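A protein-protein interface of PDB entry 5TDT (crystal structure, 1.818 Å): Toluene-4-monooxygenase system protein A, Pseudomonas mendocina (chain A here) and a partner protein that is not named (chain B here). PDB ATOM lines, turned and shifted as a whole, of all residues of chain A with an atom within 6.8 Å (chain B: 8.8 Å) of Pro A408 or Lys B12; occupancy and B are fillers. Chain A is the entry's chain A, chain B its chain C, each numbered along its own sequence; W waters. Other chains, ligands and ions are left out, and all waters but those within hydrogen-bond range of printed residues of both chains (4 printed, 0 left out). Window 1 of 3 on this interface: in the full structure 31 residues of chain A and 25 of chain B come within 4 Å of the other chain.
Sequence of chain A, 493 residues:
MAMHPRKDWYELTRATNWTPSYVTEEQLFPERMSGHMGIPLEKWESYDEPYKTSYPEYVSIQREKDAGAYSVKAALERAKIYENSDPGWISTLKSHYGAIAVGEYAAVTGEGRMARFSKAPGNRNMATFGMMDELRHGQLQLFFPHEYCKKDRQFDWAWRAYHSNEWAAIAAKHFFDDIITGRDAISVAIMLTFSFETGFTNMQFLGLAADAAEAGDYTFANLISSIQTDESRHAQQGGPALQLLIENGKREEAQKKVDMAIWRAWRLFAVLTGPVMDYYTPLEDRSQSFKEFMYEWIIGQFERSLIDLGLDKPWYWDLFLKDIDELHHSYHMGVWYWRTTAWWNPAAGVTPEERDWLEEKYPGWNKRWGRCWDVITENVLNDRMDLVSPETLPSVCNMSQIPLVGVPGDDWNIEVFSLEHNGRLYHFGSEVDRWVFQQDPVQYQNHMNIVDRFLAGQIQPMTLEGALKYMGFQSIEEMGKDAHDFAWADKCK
The side-chain sulfur of Cys A372 lies close to the backbone carbonyl oxygen of Arg B42 (3.5 Å).
The backbone carbonyl oxygen (O) of Phe B14 is in hydrogen-bond range of the backbone NH (N) of Gly A406 (2.9 Å).
The backbone carbonyl oxygen (O) of Lys B12 sits at hydrogen-bond distance from the backbone NH (N) of Gly A409, at 3.0 Å.
NE1 of Trp A412 sits close to O of Asp B13 (3.2 Å).
The side-chain hydroxyl (OG) of Ser A330 sits at hydrogen-bond distance from the indole nitrogen (NE1) of Trp A369, at 2.9 Å.
The side-chain hydroxyl (OG) of Ser A330 is in hydrogen-bond range of the backbone carbonyl oxygen (O) of Gly A406, 2.6 Å away.
The guanidinium group of Arg B46 is in salt-bridge range of the side-chain carboxylate of Glu B11, at 3.9 Å.
The backbone NH (N) of Phe B82 lies within hydrogen-bond range of the side-chain carboxylate (OE2) of Glu B11 (3.0 Å).
The side-chain carboxylate (OD1) of Asp B13 sits at hydrogen-bond distance from the side-chain sulfur (SG) of Cys B38 (3.4 Å).
OD1 of Asp B13 lies within salt-bridge range of NH1 of Arg B42.
Among the printed residues, pairs that only touch across the chains: Ser A330 with Phe B14 (3.2 Å), Met A333 with Phe B14 (3.6 Å), Pro A408 with Lys B12 (3.3 Å), Pro A408 with Asp B13 (3.4 Å), Pro A408 with Phe B14 (3.8 Å), Trp A412 with Phe B10 (3.5 Å), Trp A412 with Glu B11 (3.7 Å), Trp A412 with Lys B12 (3.2 Å) and Trp A412 with Val B81 (3.8 Å).
Of the printed residues of chain B, Met A333 touches Phe B14.
Of the printed residues of chain B, Cys A372 touches Arg B42.
Of chain B, only Lys B12, Asp B13 and Phe B14 come within 4 Å of Pro A408.
Of chain B, only Lys B12 (3.0 Å) comes within 4 Å of Gly A409.
Of chain A, only Pro A408 (3.3 Å), Gly A409 (3.0 Å) and Trp A412 (3.2 Å) come within 4 Å of Lys B12.
Val B43 touches none of the printed residues of chain A.
Pro B45 touches none of the printed residues of chain A.
The nearest residue of chain A that does not touch Lys B12 is Cys A372 (4.1 Å).
Along chain B the printed residues that touch a printed residue of chain A span positions 10 to 81.
Hydrophobic or aromatic side chains of chain A within 4 Å of the printed part of chain B: Met A333, Pro A408 and Trp A412.
Water W2 lies within hydrogen-bond range of the side-chain carboxylate of Asp A410 (2.5 Å) and the side-chain amino group of Lys B12 (3.0 Å).
Water W4 lies within hydrogen-bond range of O of Asp B13 (2.7 Å), O of Val A407 (3.1 Å) and NE1 of Trp A412 (3.4 Å).
Water W3 lies within hydrogen-bond range of O of Lys B12 (2.8 Å), O of Arg B42 (3.0 Å) and SG of Cys A372 (3.7 Å).
Water W1 lies within hydrogen-bond range of O of Phe B10, NE1 of Trp A412 and O of Leu B15.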
ATOM      1  N   SER A 330      22.534  20.082  11.818  1.00  0.00           N
ATOM      2  CA  SER A 330      22.293  21.522  11.781  1.00  0.00           C
ATOM      3  C   SER A 330      22.414  22.074  10.363  1.00  0.00           C
ATOM      4  O   SER A 330      21.630  22.943   9.966  1.00  0.00           O
ATOM      5  CB  SER A 330      23.258  22.235  12.728  1.00  0.00           C
ATOM      6  OG  SER A 330      22.900  22.006  14.082  1.00  0.00           O
ATOM      7  N   MET A 333      19.129  21.283   8.737  1.00  0.00           N
ATOM      8  CA  MET A 333      18.075  22.179   9.208  1.00  0.00           C
ATOM      9  C   MET A 333      18.191  23.540   8.546  1.00  0.00           C
ATOM     10  O   MET A 333      17.180  24.153   8.191  1.00  0.00           O
ATOM     11  CB  MET A 333      18.153  22.310  10.731  1.00  0.00           C
ATOM     12  CG  MET A 333      17.127  23.271  11.356  1.00  0.00           C
ATOM     13  SD  MET A 333      17.226  23.141  13.158  1.00  0.00           S
ATOM     14  CE  MET A 333      16.729  21.434  13.388  1.00  0.00           C
ATOM     15  N   LYS A 367      15.647  15.414  21.472  1.00  0.00           N
ATOM     16  CA  LYS A 367      15.775  16.479  22.471  1.00  0.00           C
ATOM     17  C   LYS A 367      16.690  17.611  22.011  1.00  0.00           C
ATOM     18  O   LYS A 367      16.886  18.573  22.763  1.00  0.00           O
ATOM     19  CB  LYS A 367      16.301  15.935  23.810  1.00  0.00           C
ATOM     20  CG  LYS A 367      15.339  15.073  24.638  1.00  0.00           C
ATOM     21  CD  LYS A 367      15.084  13.741  23.973  1.00  0.00           C
ATOM     22  CE  LYS A 367      16.383  13.092  23.502  1.00  0.00           C
ATOM     23  NZ  LYS A 367      16.137  12.156  22.374  1.00  0.00           N
ATOM     24  N   ARG A 368      17.249  17.518  20.800  1.00  0.00           N
ATOM     25  CA  ARG A 368      18.112  18.558  20.261  1.00  0.00           C
ATOM     26  C   ARG A 368      17.454  19.100  19.006  1.00  0.00           C
ATOM     27  O   ARG A 368      16.556  19.958  19.107  1.00  0.00           O
ATOM     28  CB  ARG A 368      19.517  17.995  20.018  1.00  0.00           C
ATOM     29  CG  ARG A 368      20.293  17.759  21.308  1.00  0.00           C
ATOM     30  CD  ARG A 368      21.484  16.838  21.050  1.00  0.00           C
ATOM     31  NE  ARG A 368      22.292  16.693  22.249  1.00  0.00           N
ATOM     32  CZ  ARG A 368      23.238  15.775  22.399  1.00  0.00           C
ATOM     33  NH1 ARG A 368      23.484  14.916  21.418  1.00  0.00           N
ATOM     34  NH2 ARG A 368      23.931  15.715  23.528  1.00  0.00           N
ATOM     35  N   TRP A 369      17.833  18.640  17.807  1.00  0.00           N
ATOM     36  CA  TRP A 369      17.214  19.129  16.582  1.00  0.00           C
ATOM     37  C   TRP A 369      15.711  18.885  16.586  1.00  0.00           C
ATOM     38  O   TRP A 369      14.957  19.668  15.998  1.00  0.00           O
ATOM     39  CB  TRP A 369      17.890  18.475  15.366  1.00  0.00           C
ATOM     40  CG  TRP A 369      19.377  18.767  15.373  1.00  0.00           C
ATOM     41  CD1 TRP A 369      20.004  19.873  14.859  1.00  0.00           C
ATOM     42  CD2 TRP A 369      20.396  17.989  16.009  1.00  0.00           C
ATOM     43  NE1 TRP A 369      21.353  19.808  15.106  1.00  0.00           N
ATOM     44  CE2 TRP A 369      21.620  18.664  15.814  1.00  0.00           C
ATOM     45  CE3 TRP A 369      20.394  16.772  16.709  1.00  0.00           C
ATOM     46  CZ2 TRP A 369      22.832  18.159  16.282  1.00  0.00           C
ATOM     47  CZ3 TRP A 369      21.596  16.278  17.178  1.00  0.00           C
ATOM     48  CH2 TRP A 369      22.797  16.973  16.968  1.00  0.00           C
ATOM     49  N   GLY A 370      15.251  17.828  17.262  1.00  0.00           N
ATOM     50  CA  GLY A 370      13.819  17.587  17.345  1.00  0.00           C
ATOM     51  C   GLY A 370      13.050  18.741  17.967  1.00  0.00           C
ATOM     52  O   GLY A 370      11.878  18.962  17.637  1.00  0.00           O
ATOM     53  N   ARG A 371      13.680  19.485  18.880  1.00  0.00           N
ATOM     54  CA  ARG A 371      12.988  20.631  19.475  1.00  0.00           C
ATOM     55  C   ARG A 371      12.672  21.690  18.425  1.00  0.00           C
ATOM     56  O   ARG A 371      11.593  22.298  18.448  1.00  0.00           O
ATOM     57  CB  ARG A 371      13.819  21.241  20.603  1.00  0.00           C
ATOM     58  CG  ARG A 371      14.072  20.304  21.775  1.00  0.00           C
ATOM     59  CD  ARG A 371      12.780  19.862  22.449  1.00  0.00           C
ATOM     60  NE  ARG A 371      13.059  19.148  23.691  1.00  0.00           N
ATOM     61  CZ  ARG A 371      12.229  18.276  24.259  1.00  0.00           C
ATOM     62  NH1 ARG A 371      11.061  17.997  23.695  1.00  0.00           N
ATOM     63  NH2 ARG A 371      12.569  17.676  25.392  1.00  0.00           N
ATOM     64  N   CYS A 372      13.603  21.938  17.500  1.00  0.00           N
ATOM     65  CA  CYS A 372      13.342  22.907  16.440  1.00  0.00           C
ATOM     66  C   CYS A 372      12.311  22.370  15.461  1.00  0.00           C
ATOM     67  O   CYS A 372      11.398  23.097  15.051  1.00  0.00           O
ATOM     68  CB  CYS A 372      14.638  23.256  15.705  1.00  0.00           C
ATOM     69  SG  CYS A 372      15.959  23.825  16.777  1.00  0.00           S
ATOM     70  N   GLY A 406      25.371  25.225  15.646  1.00  0.00           N
ATOM     71  CA  GLY A 406      25.705  24.493  16.844  1.00  0.00           C
ATOM     72  C   GLY A 406      24.617  23.479  17.130  1.00  0.00           C
ATOM     73  O   GLY A 406      23.858  23.086  16.245  1.00  0.00           O
ATOM     74  N   VAL A 407      24.519  23.070  18.385  1.00  0.00           N
ATOM     75  CA  VAL A 407      23.556  22.061  18.806  1.00  0.00           C
ATOM     76  C   VAL A 407      22.381  22.798  19.445  1.00  0.00           C
ATOM     77  O   VAL A 407      22.595  23.551  20.406  1.00  0.00           O
ATOM     78  CB  VAL A 407      24.173  21.049  19.779  1.00  0.00           C
ATOM     79  CG1 VAL A 407      23.101  20.060  20.274  1.00  0.00           C
ATOM     80  CG2 VAL A 407      25.344  20.316  19.106  1.00  0.00           C
ATOM     81  N   PRO A 408      21.154  22.624  18.943  1.00  0.00           N
ATOM     82  CA  PRO A 408      20.008  23.341  19.505  1.00  0.00           C
ATOM     83  C   PRO A 408      19.358  22.562  20.640  1.00  0.00           C
ATOM     84  O   PRO A 408      19.786  21.446  20.962  1.00  0.00           O
ATOM     85  CB  PRO A 408      19.067  23.451  18.298  1.00  0.00           C
ATOM     86  CG  PRO A 408      19.248  22.103  17.602  1.00  0.00           C
ATOM     87  CD  PRO A 408      20.757  21.771  17.805  1.00  0.00           C
ATOM     88  N   GLY A 409      18.305  23.121  21.233  1.00  0.00           N
ATOM     89  CA  GLY A 409      17.455  22.330  22.104  1.00  0.00           C
ATOM     90  C   GLY A 409      17.893  22.222  23.550  1.00  0.00           C
ATOM     91  O   GLY A 409      18.390  23.189  24.140  1.00  0.00           O
ATOM     92  N   ASP A 410      17.727  21.029  24.129  1.00  0.00           N
ATOM     93  CA  ASP A 410      17.798  20.896  25.582  1.00  0.00           C
ATOM     94  C   ASP A 410      19.196  21.178  26.139  1.00  0.00           C
ATOM     95  O   ASP A 410      19.309  21.722  27.239  1.00  0.00           O
ATOM     96  CB  ASP A 410      17.314  19.506  26.007  1.00  0.00           C
ATOM     97  CG  ASP A 410      15.810  19.336  25.857  1.00  0.00           C
ATOM     98  OD1 ASP A 410      15.124  20.293  25.437  1.00  0.00           O
ATOM     99  OD2 ASP A 410      15.310  18.242  26.187  1.00  0.00           O
ATOM    100  N   ASP A 411      20.263  20.834  25.415  1.00  0.00           N
ATOM    101  CA  ASP A 411      21.606  21.178  25.877  1.00  0.00           C
ATOM    102  C   ASP A 411      22.298  22.064  24.841  1.00  0.00           C
ATOM    103  O   ASP A 411      23.399  21.766  24.357  1.00  0.00           O
ATOM    104  CB  ASP A 411      22.433  19.928  26.207  1.00  0.00           C
ATOM    105  CG  ASP A 411      22.691  19.048  25.002  1.00  0.00           C
ATOM    106  OD1 ASP A 411      21.827  18.988  24.113  1.00  0.00           O
ATOM    107  OD2 ASP A 411      23.771  18.418  24.946  1.00  0.00           O
ATOM    108  N   TRP A 412      21.628  23.164  24.511  1.00  0.00           N
ATOM    109  CA  TRP A 412      22.110  24.167  23.575  1.00  0.00           C
ATOM    110  C   TRP A 412      23.585  24.472  23.783  1.00  0.00           C
ATOM    111  O   TRP A 412      24.022  24.748  24.902  1.00  0.00           O
ATOM    112  CB  TRP A 412      21.289  25.440  23.761  1.00  0.00           C
ATOM    113  CG  TRP A 412      21.707  26.596  22.921  1.00  0.00           C
ATOM    114  CD1 TRP A 412      21.667  26.677  21.555  1.00  0.00           C
ATOM    115  CD2 TRP A 412      22.175  27.867  23.386  1.00  0.00           C
ATOM    116  NE1 TRP A 412      22.100  27.917  21.146  1.00  0.00           N
ATOM    117  CE2 TRP A 412      22.414  28.667  22.246  1.00  0.00           C
ATOM    118  CE3 TRP A 412      22.431  28.406  24.656  1.00  0.00           C
ATOM    119  CZ2 TRP A 412      22.893  29.987  22.337  1.00  0.00           C
ATOM    120  CZ3 TRP A 412      22.908  29.724  24.743  1.00  0.00           C
ATOM    121  CH2 TRP A 412      23.132  30.489  23.592  1.00  0.00           C
ATOM    122  N   ASN A 413      24.348  24.414  22.697  1.00  0.00           N
ATOM    123  CA  ASN A 413      25.735  24.852  22.742  1.00  0.00           C
ATOM    124  C   ASN A 413      26.142  25.292  21.348  1.00  0.00           C
ATOM    125  O   ASN A 413      26.048  24.505  20.404  1.00  0.00           O
ATOM    126  CB  ASN A 413      26.662  23.743  23.246  1.00  0.00           C
ATOM    127  CG  ASN A 413      28.097  24.201  23.336  1.00  0.00           C
ATOM    128  OD1 ASN A 413      28.411  25.147  24.058  1.00  0.00           O
ATOM    129  ND2 ASN A 413      28.978  23.548  22.592  1.00  0.00           N
ATOM    130  N   ALA B   9      23.310  34.756  18.455  1.00  0.00           N
ATOM    131  CA  ALA B   9      22.910  33.376  18.701  1.00  0.00           C
ATOM    132  C   ALA B   9      21.849  33.367  19.796  1.00  0.00           C
ATOM    133  O   ALA B   9      22.122  33.799  20.915  1.00  0.00           O
ATOM    134  CB  ALA B   9      24.118  32.537  19.116  1.00  0.00           C
ATOM    135  N   PHE B  10      20.650  32.861  19.491  1.00  0.00           N
ATOM    136  CA  PHE B  10      19.569  32.826  20.480  1.00  0.00           C
ATOM    137  C   PHE B  10      19.516  31.481  21.200  1.00  0.00           C
ATOM    138  O   PHE B  10      19.667  30.429  20.575  1.00  0.00           O
ATOM    139  CB  PHE B  10      18.222  33.094  19.814  1.00  0.00           C
ATOM    140  CG  PHE B  10      17.119  33.415  20.785  1.00  0.00           C
ATOM    141  CD1 PHE B  10      16.362  32.405  21.368  1.00  0.00           C
ATOM    142  CD2 PHE B  10      16.826  34.737  21.102  1.00  0.00           C
ATOM    143  CE1 PHE B  10      15.323  32.715  22.263  1.00  0.00           C
ATOM    144  CE2 PHE B  10      15.793  35.056  21.983  1.00  0.00           C
ATOM    145  CZ  PHE B  10      15.047  34.041  22.570  1.00  0.00           C
ATOM    146  N   GLU B  11      19.269  31.526  22.514  1.00  0.00           N
ATOM    147  CA  GLU B  11      19.289  30.329  23.357  1.00  0.00           C
ATOM    148  C   GLU B  11      18.332  29.261  22.834  1.00  0.00           C
ATOM    149  O   GLU B  11      17.130  29.512  22.673  1.00  0.00           O
ATOM    150  CB  GLU B  11      18.930  30.693  24.805  1.00  0.00           C
ATOM    151  CG  GLU B  11      19.067  29.526  25.790  1.00  0.00           C
ATOM    152  CD  GLU B  11      18.815  29.910  27.249  1.00  0.00           C
ATOM    153  OE1 GLU B  11      18.042  29.207  27.931  1.00  0.00           O
ATOM    154  OE2 GLU B  11      19.389  30.901  27.723  1.00  0.00           O
ATOM    155  N   LYS B  12      18.879  28.070  22.577  1.00  0.00           N
ATOM    156  CA  LYS B  12      18.233  26.833  22.107  1.00  0.00           C
ATOM    157  C   LYS B  12      18.023  26.809  20.589  1.00  0.00           C
ATOM    158  O   LYS B  12      17.488  25.814  20.071  1.00  0.00           O
ATOM    159  CB  LYS B  12      16.897  26.546  22.820  1.00  0.00           C
ATOM    160  CG  LYS B  12      17.083  26.346  24.325  1.00  0.00           C
ATOM    161  CD  LYS B  12      15.843  25.800  25.023  1.00  0.00           C
ATOM    162  CE  LYS B  12      16.178  25.403  26.460  1.00  0.00           C
ATOM    163  NZ  LYS B  12      15.151  24.491  27.039  1.00  0.00           N
ATOM    164  N   ASP B  13      18.420  27.848  19.861  1.00  0.00           N
ATOM    165  CA  ASP B  13      18.405  27.828  18.403  1.00  0.00           C
ATOM    166  C   ASP B  13      19.618  27.033  17.890  1.00  0.00           C
ATOM    167  O   ASP B  13      20.480  26.606  18.664  1.00  0.00           O
ATOM    168  CB  ASP B  13      18.397  29.263  17.874  1.00  0.00           C
ATOM    169  CG  ASP B  13      17.769  29.394  16.483  1.00  0.00           C
ATOM    170  OD1 ASP B  13      17.696  30.544  15.981  1.00  0.00           O
ATOM    171  OD2 ASP B  13      17.373  28.372  15.884  1.00  0.00           O
ATOM    172  N   PHE B  14      19.680  26.811  16.574  1.00  0.00           N
ATOM    173  CA  PHE B  14      20.755  26.004  15.992  1.00  0.00           C
ATOM    174  C   PHE B  14      21.832  26.821  15.274  1.00  0.00           C
ATOM    175  O   PHE B  14      22.821  26.233  14.828  1.00  0.00           O
ATOM    176  CB  PHE B  14      20.190  24.966  15.010  1.00  0.00           C
ATOM    177  CG  PHE B  14      19.940  25.506  13.626  1.00  0.00           C
ATOM    178  CD1 PHE B  14      18.885  26.397  13.384  1.00  0.00           C
ATOM    179  CD2 PHE B  14      20.758  25.138  12.566  1.00  0.00           C
ATOM    180  CE1 PHE B  14      18.647  26.895  12.095  1.00  0.00           C
ATOM    181  CE2 PHE B  14      20.533  25.637  11.281  1.00  0.00           C
ATOM    182  CZ  PHE B  14      19.475  26.512  11.047  1.00  0.00           C
ATOM    183  N   LEU B  15      21.684  28.139  15.133  1.00  0.00           N
ATOM    184  CA  LEU B  15      22.630  28.879  14.303  1.00  0.00           C
ATOM    185  C   LEU B  15      22.827  30.288  14.843  1.00  0.00           C
ATOM    186  O   LEU B  15      22.132  30.737  15.767  1.00  0.00           O
ATOM    187  CB  LEU B  15      22.173  28.929  12.832  1.00  0.00           C
ATOM    188  CG  LEU B  15      21.267  30.104  12.437  1.00  0.00           C
ATOM    189  CD1 LEU B  15      21.019  30.066  10.928  1.00  0.00           C
ATOM    190  CD2 LEU B  15      19.957  30.081  13.219  1.00  0.00           C
ATOM    191  N   CYS B  38      13.621  34.009  15.745  1.00  0.00           N
ATOM    192  CA  CYS B  38      13.956  32.752  16.409  1.00  0.00           C
ATOM    193  C   CYS B  38      12.767  32.149  17.146  1.00  0.00           C
ATOM    194  O   CYS B  38      12.451  30.968  16.969  1.00  0.00           O
ATOM    195  CB  CYS B  38      15.095  32.962  17.412  1.00  0.00           C
ATOM    196  SG  CYS B  38      16.601  33.697  16.731  1.00  0.00           S
ATOM    197  N   ARG B  42      11.974  28.439  15.360  1.00  0.00           N
ATOM    198  CA  ARG B  42      12.681  27.214  15.691  1.00  0.00           C
ATOM    199  C   ARG B  42      12.843  27.059  17.198  1.00  0.00           C
ATOM    200  O   ARG B  42      13.393  26.049  17.653  1.00  0.00           O
ATOM    201  CB  ARG B  42      14.051  27.202  14.998  1.00  0.00           C
ATOM    202  CG  ARG B  42      13.993  27.293  13.462  1.00  0.00           C
ATOM    203  CD  ARG B  42      15.394  27.497  12.844  1.00  0.00           C
ATOM    204  NE  ARG B  42      16.016  28.690  13.407  1.00  0.00           N
ATOM    205  CZ  ARG B  42      15.796  29.936  12.984  1.00  0.00           C
ATOM    206  NH1 ARG B  42      16.378  30.956  13.606  1.00  0.00           N
ATOM    207  NH2 ARG B  42      14.997  30.171  11.950  1.00  0.00           N
ATOM    208  N   VAL B  43      12.371  28.028  17.983  1.00  0.00           N
ATOM    209  CA  VAL B  43      12.571  28.056  19.425  1.00  0.00           C
ATOM    210  C   VAL B  43      11.209  28.234  20.086  1.00  0.00           C
ATOM    211  O   VAL B  43      10.430  29.109  19.683  1.00  0.00           O
ATOM    212  CB  VAL B  43      13.535  29.186  19.833  1.00  0.00           C
ATOM    213  CG1 VAL B  43      13.618  29.306  21.333  1.00  0.00           C
ATOM    214  CG2 VAL B  43      14.925  28.947  19.225  1.00  0.00           C
ATOM    215  N   ALA B  44      10.929  27.415  21.095  1.00  0.00           N
ATOM    216  CA  ALA B  44       9.639  27.488  21.778  1.00  0.00           C
ATOM    217  C   ALA B  44       9.565  28.741  22.651  1.00  0.00           C
ATOM    218  O   ALA B  44      10.559  29.125  23.275  1.00  0.00           O
ATOM    219  CB  ALA B  44       9.417  26.246  22.639  1.00  0.00           C
ATOM    220  N   PRO B  45       8.410  29.402  22.716  1.00  0.00           N
ATOM    221  CA  PRO B  45       8.268  30.548  23.625  1.00  0.00           C
ATOM    222  C   PRO B  45       8.314  30.092  25.074  1.00  0.00           C
ATOM    223  O   PRO B  45       7.992  28.948  25.402  1.00  0.00           O
ATOM    224  CB  PRO B  45       6.886  31.126  23.281  1.00  0.00           C
ATOM    225  CG  PRO B  45       6.356  30.308  22.150  1.00  0.00           C
ATOM    226  CD  PRO B  45       7.142  29.047  22.061  1.00  0.00           C
ATOM    227  N   ARG B  46       8.701  31.018  25.954  1.00  0.00           N
ATOM    228  CA  ARG B  46       8.836  30.692  27.369  1.00  0.00           C
ATOM    229  C   ARG B  46       8.770  31.957  28.212  1.00  0.00           C
ATOM    230  O   ARG B  46       9.084  33.058  27.748  1.00  0.00           O
ATOM    231  CB  ARG B  46      10.147  29.951  27.659  1.00  0.00           C
ATOM    232  CG  ARG B  46      11.405  30.678  27.178  1.00  0.00           C
ATOM    233  CD  ARG B  46      12.651  30.184  27.913  1.00  0.00           C
ATOM    234  NE  ARG B  46      12.679  30.659  29.294  1.00  0.00           N
ATOM    235  CZ  ARG B  46      13.643  30.380  30.169  1.00  0.00           C
ATOM    236  NH1 ARG B  46      13.577  30.854  31.406  1.00  0.00           N
ATOM    237  NH2 ARG B  46      14.668  29.619  29.813  1.00  0.00           N
ATOM    238  N   VAL B  80      21.757  35.863  23.102  1.00  0.00           N
ATOM    239  CA  VAL B  80      20.520  36.251  23.783  1.00  0.00           C
ATOM    240  C   VAL B  80      20.049  35.039  24.577  1.00  0.00           C
ATOM    241  O   VAL B  80      19.747  33.986  23.995  1.00  0.00           O
ATOM    242  CB  VAL B  80      19.433  36.719  22.803  1.00  0.00           C
ATOM    243  CG1 VAL B  80      18.188  37.165  23.580  1.00  0.00           C
ATOM    244  CG2 VAL B  80      19.961  37.845  21.904  1.00  0.00           C
ATOM    245  N   VAL B  81      20.006  35.184  25.902  1.00  0.00           N
ATOM    246  CA  VAL B  81      19.776  34.082  26.828  1.00  0.00           C
ATOM    247  C   VAL B  81      18.781  34.534  27.889  1.00  0.00           C
ATOM    248  O   VAL B  81      18.452  35.722  28.009  1.00  0.00           O
ATOM    249  CB  VAL B  81      21.082  33.609  27.512  1.00  0.00           C
ATOM    250  CG1 VAL B  81      22.077  33.051  26.488  1.00  0.00           C
ATOM    251  CG2 VAL B  81      21.699  34.758  28.304  1.00  0.00           C
ATOM    252  N   PHE B  82      18.316  33.562  28.676  1.00  0.00           N
ATOM    253  CA  PHE B  82      17.408  33.801  29.791  1.00  0.00           C
ATOM    254  C   PHE B  82      18.152  33.638  31.108  1.00  0.00           C
ATOM    255  O   PHE B  82      19.025  32.774  31.238  1.00  0.00           O
ATOM    256  CB  PHE B  82      16.205  32.845  29.744  1.00  0.00           C
ATOM    257  CG  PHE B  82      15.254  33.119  28.607  1.00  0.00           C
ATOM    258  CD1 PHE B  82      15.446  32.531  27.371  1.00  0.00           C
ATOM    259  CD2 PHE B  82      14.180  33.973  28.775  1.00  0.00           C
ATOM    260  CE1 PHE B  82      14.579  32.781  26.329  1.00  0.00           C
ATOM    261  CE2 PHE B  82      13.307  34.231  27.735  1.00  0.00           C
ATOM    262  CZ  PHE B  82      13.504  33.636  26.508  1.00  0.00           C
HETATM  263  O   HOH W   1      21.900  29.824  18.777  1.00  0.00           O
HETATM  264  O   HOH W   2      14.696  22.680  24.690  1.00  0.00           O
HETATM  265  O   HOH W   3      14.756  25.024  20.075  1.00  0.00           O
HETATM  266  O   HOH W   4      23.080  25.951  18.561  1.00  0.00           O
